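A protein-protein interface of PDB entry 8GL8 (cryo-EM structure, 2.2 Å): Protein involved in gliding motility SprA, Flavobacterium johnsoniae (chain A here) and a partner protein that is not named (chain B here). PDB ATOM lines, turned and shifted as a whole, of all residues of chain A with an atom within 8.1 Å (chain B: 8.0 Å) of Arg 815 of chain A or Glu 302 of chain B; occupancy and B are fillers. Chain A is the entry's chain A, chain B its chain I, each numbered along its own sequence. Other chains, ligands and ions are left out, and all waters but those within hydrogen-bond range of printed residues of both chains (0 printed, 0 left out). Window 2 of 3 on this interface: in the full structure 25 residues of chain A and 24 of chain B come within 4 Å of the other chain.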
ATOM      1  N   VAL A 810      20.228  35.994  -6.377  1.00  0.00           N
ATOM      2  CA  VAL A 810      19.157  35.004  -6.312  1.00  0.00           C
ATOM      3  C   VAL A 810      19.751  33.611  -6.491  1.00  0.00           C
ATOM      4  O   VAL A 810      19.910  33.147  -7.628  1.00  0.00           O
ATOM      5  CB  VAL A 810      18.073  35.284  -7.365  1.00  0.00           C
ATOM      6  CG1 VAL A 810      16.930  34.289  -7.230  1.00  0.00           C
ATOM      7  CG2 VAL A 810      17.563  36.709  -7.236  1.00  0.00           C
ATOM      8  N   PRO A 811      20.095  32.915  -5.405  1.00  0.00           N
ATOM      9  CA  PRO A 811      20.593  31.536  -5.544  1.00  0.00           C
ATOM     10  C   PRO A 811      19.554  30.571  -6.083  1.00  0.00           C
ATOM     11  O   PRO A 811      19.922  29.491  -6.565  1.00  0.00           O
ATOM     12  CB  PRO A 811      21.012  31.171  -4.114  1.00  0.00           C
ATOM     13  CG  PRO A 811      20.183  32.055  -3.246  1.00  0.00           C
ATOM     14  CD  PRO A 811      20.028  33.342  -3.998  1.00  0.00           C
ATOM     15  N   PHE A 812      18.268  30.923  -6.009  1.00  0.00           N
ATOM     16  CA  PHE A 812      17.223  30.050  -6.529  1.00  0.00           C
ATOM     17  C   PHE A 812      17.368  29.853  -8.033  1.00  0.00           C
ATOM     18  O   PHE A 812      17.119  28.758  -8.550  1.00  0.00           O
ATOM     19  CB  PHE A 812      15.850  30.626  -6.184  1.00  0.00           C
ATOM     20  CG  PHE A 812      14.733  30.086  -7.028  1.00  0.00           C
ATOM     21  CD1 PHE A 812      14.171  28.851  -6.745  1.00  0.00           C
ATOM     22  CD2 PHE A 812      14.233  30.816  -8.094  1.00  0.00           C
ATOM     23  CE1 PHE A 812      13.139  28.352  -7.516  1.00  0.00           C
ATOM     24  CE2 PHE A 812      13.204  30.320  -8.869  1.00  0.00           C
ATOM     25  CZ  PHE A 812      12.655  29.087  -8.579  1.00  0.00           C
ATOM     26  N   LEU A 813      17.763  30.904  -8.754  1.00  0.00           N
ATOM     27  CA  LEU A 813      17.970  30.775 -10.192  1.00  0.00           C
ATOM     28  C   LEU A 813      19.129  29.834 -10.504  1.00  0.00           C
ATOM     29  O   LEU A 813      19.053  29.042 -11.449  1.00  0.00           O
ATOM     30  CB  LEU A 813      18.205  32.151 -10.814  1.00  0.00           C
ATOM     31  CG  LEU A 813      16.962  33.026 -10.985  1.00  0.00           C
ATOM     32  CD1 LEU A 813      17.317  34.334 -11.670  1.00  0.00           C
ATOM     33  CD2 LEU A 813      15.885  32.284 -11.759  1.00  0.00           C
ATOM     34  N   THR A 814      20.209  29.904  -9.721  1.00  0.00           N
ATOM     35  CA  THR A 814      21.314  28.968  -9.906  1.00  0.00           C
ATOM     36  C   THR A 814      20.882  27.539  -9.601  1.00  0.00           C
ATOM     37  O   THR A 814      21.274  26.598 -10.304  1.00  0.00           O
ATOM     38  CB  THR A 814      22.498  29.367  -9.027  1.00  0.00           C
ATOM     39  OG1 THR A 814      22.805  30.751  -9.235  1.00  0.00           O
ATOM     40  CG2 THR A 814      23.721  28.529  -9.367  1.00  0.00           C
ATOM     41  N   ARG A 815      20.072  27.355  -8.556  1.00  0.00           N
ATOM     42  CA  ARG A 815      19.565  26.025  -8.240  1.00  0.00           C
ATOM     43  C   ARG A 815      18.696  25.485  -9.369  1.00  0.00           C
ATOM     44  O   ARG A 815      18.773  24.299  -9.710  1.00  0.00           O
ATOM     45  CB  ARG A 815      18.780  26.061  -6.930  1.00  0.00           C
ATOM     46  CG  ARG A 815      19.648  26.157  -5.689  1.00  0.00           C
ATOM     47  CD  ARG A 815      18.813  26.036  -4.427  1.00  0.00           C
ATOM     48  NE  ARG A 815      18.573  27.332  -3.804  1.00  0.00           N
ATOM     49  CZ  ARG A 815      17.371  27.851  -3.599  1.00  0.00           C
ATOM     50  NH1 ARG A 815      16.272  27.215  -3.967  1.00  0.00           N
ATOM     51  NH2 ARG A 815      17.270  29.039  -3.010  1.00  0.00           N
ATOM     52  N   LEU A 816      17.854  26.340  -9.953  1.00  0.00           N
ATOM     53  CA  LEU A 816      17.034  25.926 -11.087  1.00  0.00           C
ATOM     54  C   LEU A 816      17.895  25.587 -12.297  1.00  0.00           C
ATOM     55  O   LEU A 816      17.606  24.628 -13.022  1.00  0.00           O
ATOM     56  CB  LEU A 816      16.029  27.025 -11.432  1.00  0.00           C
ATOM     57  CG  LEU A 816      14.701  26.584 -12.051  1.00  0.00           C
ATOM     58  CD1 LEU A 816      13.599  27.566 -11.692  1.00  0.00           C
ATOM     59  CD2 LEU A 816      14.820  26.448 -13.561  1.00  0.00           C
ATOM     60  N   ALA A 817      18.950  26.369 -12.535  1.00  0.00           N
ATOM     61  CA  ALA A 817      19.852  26.081 -13.645  1.00  0.00           C
ATOM     62  C   ALA A 817      20.549  24.743 -13.453  1.00  0.00           C
ATOM     63  O   ALA A 817      20.770  24.005 -14.421  1.00  0.00           O
ATOM     64  CB  ALA A 817      20.876  27.203 -13.795  1.00  0.00           C
ATOM     65  N   ASN A 818      20.905  24.409 -12.212  1.00  0.00           N
ATOM     66  CA  ASN A 818      21.540  23.126 -11.942  1.00  0.00           C
ATOM     67  C   ASN A 818      20.588  21.949 -12.106  1.00  0.00           C
ATOM     68  O   ASN A 818      21.049  20.803 -12.123  1.00  0.00           O
ATOM     69  CB  ASN A 818      22.139  23.127 -10.536  1.00  0.00           C
ATOM     70  CG  ASN A 818      23.445  23.891 -10.466  1.00  0.00           C
ATOM     71  OD1 ASN A 818      24.358  23.650 -11.254  1.00  0.00           O
ATOM     72  ND2 ASN A 818      23.539  24.818  -9.523  1.00  0.00           N
ATOM     73  N   LYS A 819      19.286  22.196 -12.229  1.00  0.00           N
ATOM     74  CA  LYS A 819      18.317  21.151 -12.522  1.00  0.00           C
ATOM     75  C   LYS A 819      18.185  20.874 -14.014  1.00  0.00           C
ATOM     76  O   LYS A 819      17.442  19.965 -14.399  1.00  0.00           O
ATOM     77  CB  LYS A 819      16.946  21.523 -11.948  1.00  0.00           C
ATOM     78  CG  LYS A 819      16.810  21.280 -10.456  1.00  0.00           C
ATOM     79  CD  LYS A 819      15.830  22.255  -9.826  1.00  0.00           C
ATOM     80  CE  LYS A 819      15.544  21.891  -8.379  1.00  0.00           C
ATOM     81  NZ  LYS A 819      16.698  22.202  -7.491  1.00  0.00           N
ATOM     82  N   LEU A 820      18.877  21.633 -14.854  1.00  0.00           N
ATOM     83  CA  LEU A 820      18.838  21.441 -16.292  1.00  0.00           C
ATOM     84  C   LEU A 820      19.689  20.238 -16.693  1.00  0.00           C
ATOM     85  O   LEU A 820      20.585  19.828 -15.951  1.00  0.00           O
ATOM     86  CB  LEU A 820      19.309  22.713 -16.992  1.00  0.00           C
ATOM     87  CG  LEU A 820      18.317  23.870 -16.841  1.00  0.00           C
ATOM     88  CD1 LEU A 820      18.848  25.146 -17.466  1.00  0.00           C
ATOM     89  CD2 LEU A 820      16.967  23.501 -17.436  1.00  0.00           C
ATOM     90  N   ILE A 823      23.866  20.788 -16.982  1.00  0.00           N
ATOM     91  CA  ILE A 823      24.427  21.979 -16.356  1.00  0.00           C
ATOM     92  C   ILE A 823      24.767  21.649 -14.909  1.00  0.00           C
ATOM     93  O   ILE A 823      23.907  21.192 -14.146  1.00  0.00           O
ATOM     94  CB  ILE A 823      23.461  23.171 -16.445  1.00  0.00           C
ATOM     95  CG1 ILE A 823      23.432  23.712 -17.876  1.00  0.00           C
ATOM     96  CG2 ILE A 823      23.867  24.261 -15.470  1.00  0.00           C
ATOM     97  CD1 ILE A 823      22.351  24.729 -18.124  1.00  0.00           C
ATOM     98  N   THR A 825      26.761  24.110 -13.035  1.00  0.00           N
ATOM     99  CA  THR A 825      27.449  25.372 -12.832  1.00  0.00           C
ATOM    100  C   THR A 825      27.392  25.799 -11.367  1.00  0.00           C
ATOM    101  O   THR A 825      26.632  25.262 -10.556  1.00  0.00           O
ATOM    102  CB  THR A 825      26.838  26.455 -13.717  1.00  0.00           C
ATOM    103  OG1 THR A 825      27.616  27.652 -13.618  1.00  0.00           O
ATOM    104  CG2 THR A 825      25.416  26.745 -13.278  1.00  0.00           C
ATOM    105  N   ASP A 826      28.217  26.793 -11.033  1.00  0.00           N
ATOM    106  CA  ASP A 826      28.256  27.349  -9.690  1.00  0.00           C
ATOM    107  C   ASP A 826      28.314  28.870  -9.660  1.00  0.00           C
ATOM    108  O   ASP A 826      28.376  29.443  -8.566  1.00  0.00           O
ATOM    109  CB  ASP A 826      29.455  26.789  -8.911  1.00  0.00           C
ATOM    110  CG  ASP A 826      29.089  25.590  -8.058  1.00  0.00           C
ATOM    111  OD1 ASP A 826      28.165  25.710  -7.227  1.00  0.00           O
ATOM    112  OD2 ASP A 826      29.727  24.528  -8.218  1.00  0.00           O
ATOM    113  N   VAL A 827      28.303  29.536 -10.809  1.00  0.00           N
ATOM    114  CA  VAL A 827      28.398  31.002 -10.812  1.00  0.00           C
ATOM    115  C   VAL A 827      27.112  31.590 -10.242  1.00  0.00           C
ATOM    116  O   VAL A 827      26.029  31.006 -10.432  1.00  0.00           O
ATOM    117  CB  VAL A 827      28.681  31.523 -12.228  1.00  0.00           C
ATOM    118  CG1 VAL A 827      29.104  30.387 -13.144  1.00  0.00           C
ATOM    119  CG2 VAL A 827      27.485  32.272 -12.806  1.00  0.00           C
ATOM    120  N   SER A 829      23.729  33.785  -9.583  1.00  0.00           N
ATOM    121  CA  SER A 829      22.673  34.405 -10.367  1.00  0.00           C
ATOM    122  C   SER A 829      22.257  35.709  -9.701  1.00  0.00           C
ATOM    123  O   SER A 829      22.099  35.766  -8.478  1.00  0.00           O
ATOM    124  CB  SER A 829      21.470  33.473 -10.495  1.00  0.00           C
ATOM    125  OG  SER A 829      21.789  32.335 -11.273  1.00  0.00           O
ATOM    126  N   MET A1529      21.163  34.223 -14.921  1.00  0.00           N
ATOM    127  CA  MET A1529      20.862  32.906 -14.374  1.00  0.00           C
ATOM    128  C   MET A1529      22.068  32.008 -14.634  1.00  0.00           C
ATOM    129  O   MET A1529      22.199  31.428 -15.719  1.00  0.00           O
ATOM    130  CB  MET A1529      19.579  32.349 -14.999  1.00  0.00           C
ATOM    131  CG  MET A1529      19.201  30.939 -14.576  1.00  0.00           C
ATOM    132  SD  MET A1529      17.693  30.405 -15.414  1.00  0.00           S
ATOM    133  CE  MET A1529      17.778  28.631 -15.206  1.00  0.00           C
ATOM    134  N   ALA A1530      22.970  31.971 -13.649  1.00  0.00           N
ATOM    135  CA  ALA A1530      24.007  30.947 -13.496  1.00  0.00           C
ATOM    136  C   ALA A1530      24.767  30.682 -14.793  1.00  0.00           C
ATOM    137  O   ALA A1530      24.884  29.545 -15.248  1.00  0.00           O
ATOM    138  CB  ALA A1530      23.403  29.655 -12.949  1.00  0.00           C
ATOM    139  N   ASN B 261      14.874  26.381   6.846  1.00  0.00           N
ATOM    140  CA  ASN B 261      15.677  25.834   5.756  1.00  0.00           C
ATOM    141  C   ASN B 261      16.743  26.785   5.226  1.00  0.00           C
ATOM    142  O   ASN B 261      17.938  26.524   5.383  1.00  0.00           O
ATOM    143  CB  ASN B 261      14.739  25.418   4.616  1.00  0.00           C
ATOM    144  CG  ASN B 261      15.440  24.642   3.513  1.00  0.00           C
ATOM    145  OD1 ASN B 261      16.664  24.543   3.476  1.00  0.00           O
ATOM    146  ND2 ASN B 261      14.653  24.089   2.600  1.00  0.00           N
ATOM    147  N   ARG B 262      16.345  27.903   4.629  1.00  0.00           N
ATOM    148  CA  ARG B 262      17.310  28.788   3.993  1.00  0.00           C
ATOM    149  C   ARG B 262      17.428  30.132   4.696  1.00  0.00           C
ATOM    150  O   ARG B 262      18.055  31.049   4.158  1.00  0.00           O
ATOM    151  CB  ARG B 262      16.958  28.981   2.519  1.00  0.00           C
ATOM    152  CG  ARG B 262      17.842  28.174   1.585  1.00  0.00           C
ATOM    153  CD  ARG B 262      17.122  27.817   0.301  1.00  0.00           C
ATOM    154  NE  ARG B 262      17.642  26.591  -0.291  1.00  0.00           N
ATOM    155  CZ  ARG B 262      16.885  25.602  -0.743  1.00  0.00           C
ATOM    156  NH1 ARG B 262      15.565  25.662  -0.691  1.00  0.00           N
ATOM    157  NH2 ARG B 262      17.466  24.526  -1.264  1.00  0.00           N
ATOM    158  N   ALA B 264      19.086  30.545   7.426  1.00  0.00           N
ATOM    159  CA  ALA B 264      20.321  30.534   8.193  1.00  0.00           C
ATOM    160  C   ALA B 264      21.377  29.752   7.426  1.00  0.00           C
ATOM    161  O   ALA B 264      21.118  29.207   6.349  1.00  0.00           O
ATOM    162  CB  ALA B 264      20.093  29.943   9.584  1.00  0.00           C
ATOM    163  N   ARG B 266      23.741  26.877   6.162  1.00  0.00           N
ATOM    164  CA  ARG B 266      23.458  25.464   5.937  1.00  0.00           C
ATOM    165  C   ARG B 266      24.232  24.551   6.874  1.00  0.00           C
ATOM    166  O   ARG B 266      23.883  23.370   6.984  1.00  0.00           O
ATOM    167  CB  ARG B 266      23.769  25.082   4.492  1.00  0.00           C
ATOM    168  CG  ARG B 266      22.587  25.211   3.563  1.00  0.00           C
ATOM    169  CD  ARG B 266      22.324  23.932   2.797  1.00  0.00           C
ATOM    170  NE  ARG B 266      20.967  23.921   2.266  1.00  0.00           N
ATOM    171  CZ  ARG B 266      20.299  22.828   1.930  1.00  0.00           C
ATOM    172  NH1 ARG B 266      20.843  21.628   2.033  1.00  0.00           N
ATOM    173  NH2 ARG B 266      19.054  22.941   1.479  1.00  0.00           N
ATOM    174  N   MET B 269      21.843  23.275   9.613  1.00  0.00           N
ATOM    175  CA  MET B 269      20.916  22.239   9.166  1.00  0.00           C
ATOM    176  C   MET B 269      21.634  20.917   8.920  1.00  0.00           C
ATOM    177  O   MET B 269      21.142  19.852   9.315  1.00  0.00           O
ATOM    178  CB  MET B 269      20.195  22.683   7.897  1.00  0.00           C
ATOM    179  CG  MET B 269      19.452  21.547   7.211  1.00  0.00           C
ATOM    180  SD  MET B 269      18.804  21.934   5.580  1.00  0.00           S
ATOM    181  CE  MET B 269      19.012  23.701   5.569  1.00  0.00           C
ATOM    182  N   MET B 270      22.795  20.960   8.265  1.00  0.00           N
ATOM    183  CA  MET B 270      23.504  19.722   7.961  1.00  0.00           C
ATOM    184  C   MET B 270      23.989  19.035   9.231  1.00  0.00           C
ATOM    185  O   MET B 270      23.875  17.810   9.368  1.00  0.00           O
ATOM    186  CB  MET B 270      24.666  20.008   7.015  1.00  0.00           C
ATOM    187  CG  MET B 270      24.244  20.112   5.563  1.00  0.00           C
ATOM    188  SD  MET B 270      23.081  18.826   5.085  1.00  0.00           S
ATOM    189  CE  MET B 270      21.630  19.806   4.732  1.00  0.00           C
ATOM    190  N   LEU B 297      19.557  13.254   1.160  1.00  0.00           N
ATOM    191  CA  LEU B 297      20.423  14.337   1.619  1.00  0.00           C
ATOM    192  C   LEU B 297      21.760  14.323   0.893  1.00  0.00           C
ATOM    193  O   LEU B 297      22.251  15.367   0.450  1.00  0.00           O
ATOM    194  CB  LEU B 297      20.651  14.214   3.121  1.00  0.00           C
ATOM    195  CG  LEU B 297      19.711  14.958   4.054  1.00  0.00           C
ATOM    196  CD1 LEU B 297      20.128  14.655   5.467  1.00  0.00           C
ATOM    197  CD2 LEU B 297      19.764  16.442   3.778  1.00  0.00           C
ATOM    198  N   ALA B 299      22.611  12.959  -1.936  1.00  0.00           N
ATOM    199  CA  ALA B 299      22.510  13.083  -3.389  1.00  0.00           C
ATOM    200  C   ALA B 299      21.990  14.454  -3.793  1.00  0.00           C
ATOM    201  O   ALA B 299      21.242  14.588  -4.764  1.00  0.00           O
ATOM    202  CB  ALA B 299      21.621  11.981  -3.957  1.00  0.00           C
ATOM    203  N   ASP B 300      22.375  15.490  -3.054  1.00  0.00           N
ATOM    204  CA  ASP B 300      21.931  16.855  -3.293  1.00  0.00           C
ATOM    205  C   ASP B 300      23.140  17.739  -3.552  1.00  0.00           C
ATOM    206  O   ASP B 300      24.183  17.587  -2.909  1.00  0.00           O
ATOM    207  CB  ASP B 300      21.134  17.387  -2.097  1.00  0.00           C
ATOM    208  CG  ASP B 300      20.298  18.602  -2.443  1.00  0.00           C
ATOM    209  OD1 ASP B 300      20.709  19.388  -3.323  1.00  0.00           O
ATOM    210  OD2 ASP B 300      19.226  18.775  -1.829  1.00  0.00           O
ATOM    211  N   ARG B 301      22.996  18.665  -4.501  1.00  0.00           N
ATOM    212  CA  ARG B 301      24.103  19.544  -4.858  1.00  0.00           C
ATOM    213  C   ARG B 301      24.350  20.618  -3.806  1.00  0.00           C
ATOM    214  O   ARG B 301      25.496  21.031  -3.605  1.00  0.00           O
ATOM    215  CB  ARG B 301      23.839  20.186  -6.221  1.00  0.00           C
ATOM    216  CG  ARG B 301      24.900  21.176  -6.655  1.00  0.00           C
ATOM    217  CD  ARG B 301      24.655  21.680  -8.064  1.00  0.00           C
ATOM    218  NE  ARG B 301      25.896  21.783  -8.821  1.00  0.00           N
ATOM    219  CZ  ARG B 301      26.827  22.705  -8.614  1.00  0.00           C
ATOM    220  NH1 ARG B 301      26.685  23.634  -7.684  1.00  0.00           N
ATOM    221  NH2 ARG B 301      27.927  22.694  -9.360  1.00  0.00           N
ATOM    222  N   GLU B 302      23.300  21.081  -3.128  1.00  0.00           N
ATOM    223  CA  GLU B 302      23.460  22.122  -2.122  1.00  0.00           C
ATOM    224  C   GLU B 302      24.158  21.630  -0.862  1.00  0.00           C
ATOM    225  O   GLU B 302      24.575  22.457  -0.046  1.00  0.00           O
ATOM    226  CB  GLU B 302      22.096  22.709  -1.758  1.00  0.00           C
ATOM    227  CG  GLU B 302      22.079  24.223  -1.656  1.00  0.00           C
ATOM    228  CD  GLU B 302      20.691  24.769  -1.392  1.00  0.00           C
ATOM    229  OE1 GLU B 302      19.708  24.091  -1.754  1.00  0.00           O
ATOM    230  OE2 GLU B 302      20.584  25.875  -0.822  1.00  0.00           O
ATOM    231  N   ASN B 303      24.299  20.318  -0.687  1.00  0.00           N
ATOM    232  CA  ASN B 303      24.873  19.740   0.520  1.00  0.00           C
ATOM    233  C   ASN B 303      26.326  19.321   0.347  1.00  0.00           C
ATOM    234  O   ASN B 303      26.884  18.697   1.253  1.00  0.00           O
ATOM    235  CB  ASN B 303      24.046  18.537   0.969  1.00  0.00           C
ATOM    236  CG  ASN B 303      22.595  18.882   1.190  1.00  0.00           C
ATOM    237  OD1 ASN B 303      22.248  20.042   1.380  1.00  0.00           O
ATOM    238  ND2 ASN B 303      21.736  17.875   1.166  1.00  0.00           N
ATOM    239  N   ARG B 304      26.949  19.650  -0.784  1.00  0.00           N
ATOM    240  CA  ARG B 304      28.301  19.165  -1.060  1.00  0.00           C
ATOM    241  C   ARG B 304      29.314  19.538   0.016  1.00  0.00           C
ATOM    242  O   ARG B 304      30.037  18.638   0.480  1.00  0.00           O
ATOM    243  CB  ARG B 304      28.753  19.658  -2.439  1.00  0.00           C
ATOM    244  CG  ARG B 304      27.950  19.087  -3.589  1.00  0.00           C
ATOM    245  CD  ARG B 304      28.824  18.298  -4.541  1.00  0.00           C
ATOM    246  NE  ARG B 304      28.166  18.081  -5.823  1.00  0.00           N
ATOM    247  CZ  ARG B 304      28.302  18.873  -6.877  1.00  0.00           C
ATOM    248  NH1 ARG B 304      29.070  19.949  -6.839  1.00  0.00           N
ATOM    249  NH2 ARG B 304      27.649  18.579  -7.997  1.00  0.00           N
ATOM    250  N   PRO B 305      29.411  20.790   0.481  1.00  0.00           N
ATOM    251  CA  PRO B 305      30.445  21.117   1.477  1.00  0.00           C
ATOM    252  C   PRO B 305      30.319  20.337   2.771  1.00  0.00           C
ATOM    253  O   PRO B 305      31.263  20.345   3.571  1.00  0.00           O
ATOM    254  CB  PRO B 305      30.243  22.619   1.720  1.00  0.00           C
ATOM    255  CG  PRO B 305      29.534  23.106   0.519  1.00  0.00           C
ATOM    256  CD  PRO B 305      28.641  21.989   0.104  1.00  0.00           C
ATOM    257  N   TYR B 306      29.192  19.671   3.007  1.00  0.00           N
ATOM    258  CA  TYR B 306      28.968  18.906   4.222  1.00  0.00           C
ATOM    259  C   TYR B 306      28.826  17.415   3.952  1.00  0.00           C
ATOM    260  O   TYR B 306      28.510  16.658   4.877  1.00  0.00           O
ATOM    261  CB  TYR B 306      27.734  19.439   4.948  1.00  0.00           C
ATOM    262  CG  TYR B 306      27.640  20.946   4.907  1.00  0.00           C
ATOM    263  CD1 TYR B 306      28.312  21.726   5.833  1.00  0.00           C
ATOM    264  CD2 TYR B 306      26.899  21.586   3.925  1.00  0.00           C
ATOM    265  CE1 TYR B 306      28.238  23.100   5.791  1.00  0.00           C
ATOM    266  CE2 TYR B 306      26.818  22.957   3.875  1.00  0.00           C
ATOM    267  CZ  TYR B 306      27.489  23.710   4.810  1.00  0.00           C
ATOM    268  OH  TYR B 306      27.412  25.083   4.762  1.00  0.00           O
ATOM    269  N   TYR B 307      29.082  16.976   2.714  1.00  0.00           N
ATOM    270  CA  TYR B 307      28.948  15.562   2.372  1.00  0.00           C
ATOM    271  C   TYR B 307      29.709  14.686   3.354  1.00  0.00           C
ATOM    272  O   TYR B 307      29.173  13.696   3.866  1.00  0.00           O
ATOM    273  CB  TYR B 307      29.452  15.316   0.952  1.00  0.00           C
ATOM    274  CG  TYR B 307      28.399  15.425  -0.120  1.00  0.00           C
ATOM    275  CD1 TYR B 307      27.124  15.875   0.173  1.00  0.00           C
ATOM    276  CD2 TYR B 307      28.686  15.081  -1.431  1.00  0.00           C
ATOM    277  CE1 TYR B 307      26.164  15.979  -0.807  1.00  0.00           C
ATOM    278  CE2 TYR B 307      27.734  15.180  -2.417  1.00  0.00           C
ATOM    279  CZ  TYR B 307      26.475  15.631  -2.101  1.00  0.00           C
ATOM    280  OH  TYR B 307      25.521  15.730  -3.086  1.00  0.00           O
ATOM    281  N   LEU B 310      27.914  14.159   6.500  1.00  0.00           N
ATOM    282  CA  LEU B 310      26.829  13.214   6.278  1.00  0.00           C
ATOM    283  C   LEU B 310      27.378  11.814   6.049  1.00  0.00           C
ATOM    284  O   LEU B 310      26.926  10.852   6.680  1.00  0.00           O
ATOM    285  CB  LEU B 310      25.975  13.666   5.097  1.00  0.00           C
ATOM    286  CG  LEU B 310      25.258  14.999   5.308  1.00  0.00           C
ATOM    287  CD1 LEU B 310      24.564  15.444   4.035  1.00  0.00           C
ATOM    288  CD2 LEU B 310      24.273  14.891   6.458  1.00  0.00           C
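The backbone carbonyl oxygen of Thr 825 of chain A is in hydrogen-bond range of the guanidinium group of Arg 301 of chain B. NE of Arg 815 of chain A lies within salt-bridge range of OE2 of Glu 302 of chain B, 3.9 Å away. OD1 of Asp 826 of chain A lies within salt-bridge range of NH1 of Arg 301 of chain B. OD1 of Asn 818 of chain A sits at hydrogen-bond distance from NE of Arg 301 of chain B.
The backbone carbonyl oxygen (O) of Thr 814 of chain A is in hydrogen-bond range of the side-chain amide nitrogen (ND2) of Asn 818 of chain A (3.0 Å). The guanidinium group (NE) of Arg 262 of chain B is in salt-bridge range of the side-chain carboxylate (OE2) of Glu 302 of chain B (3.1 Å). The backbone NH of Val 827 of chain A sits close to the side-chain hydroxyl of Thr 825 of chain A. The side-chain carboxylate (OE1) of Glu 302 of chain B is in salt-bridge range of the guanidinium group (NH2) of Arg 266 of chain B (3.5 Å). OD1 of Asp 300 of chain B lies within hydrogen-bond range of N of Glu 302 of chain B (3.1 Å). The side-chain amide oxygen of Asn 818 of chain A lies close to the backbone carbonyl oxygen of Thr 825 of chain A (2.9 Å).
Among the printed residues, merely in contact across the chains: Arg 815 of chain A with Arg 262 of chain B.
Arg 815 of chain A touches just these residues of chain B: Arg 262 (3.5 Å) and Glu 302 (3.4 Å). Printed residues of chain B within 4 Å of Asp 826 of chain A: Arg 301. Printed residues of chain A within 4 Å of Arg 262 of chain B: Arg 815. Printed residues of chain A within 4 Å of Arg 301 of chain B: Asn 818 (3.4 Å), Thr 825 (3.1 Å) and Asp 826 (2.6 Å). Glu 302 of chain B touches just one residue of chain A: Arg 815.
Of the 18 printed residues of chain A, 4 touch a printed residue of chain B. Printed residues of chain A that touch a printed residue of chain B: Arg 815, Asn 818, Thr 825 and Asp 826.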
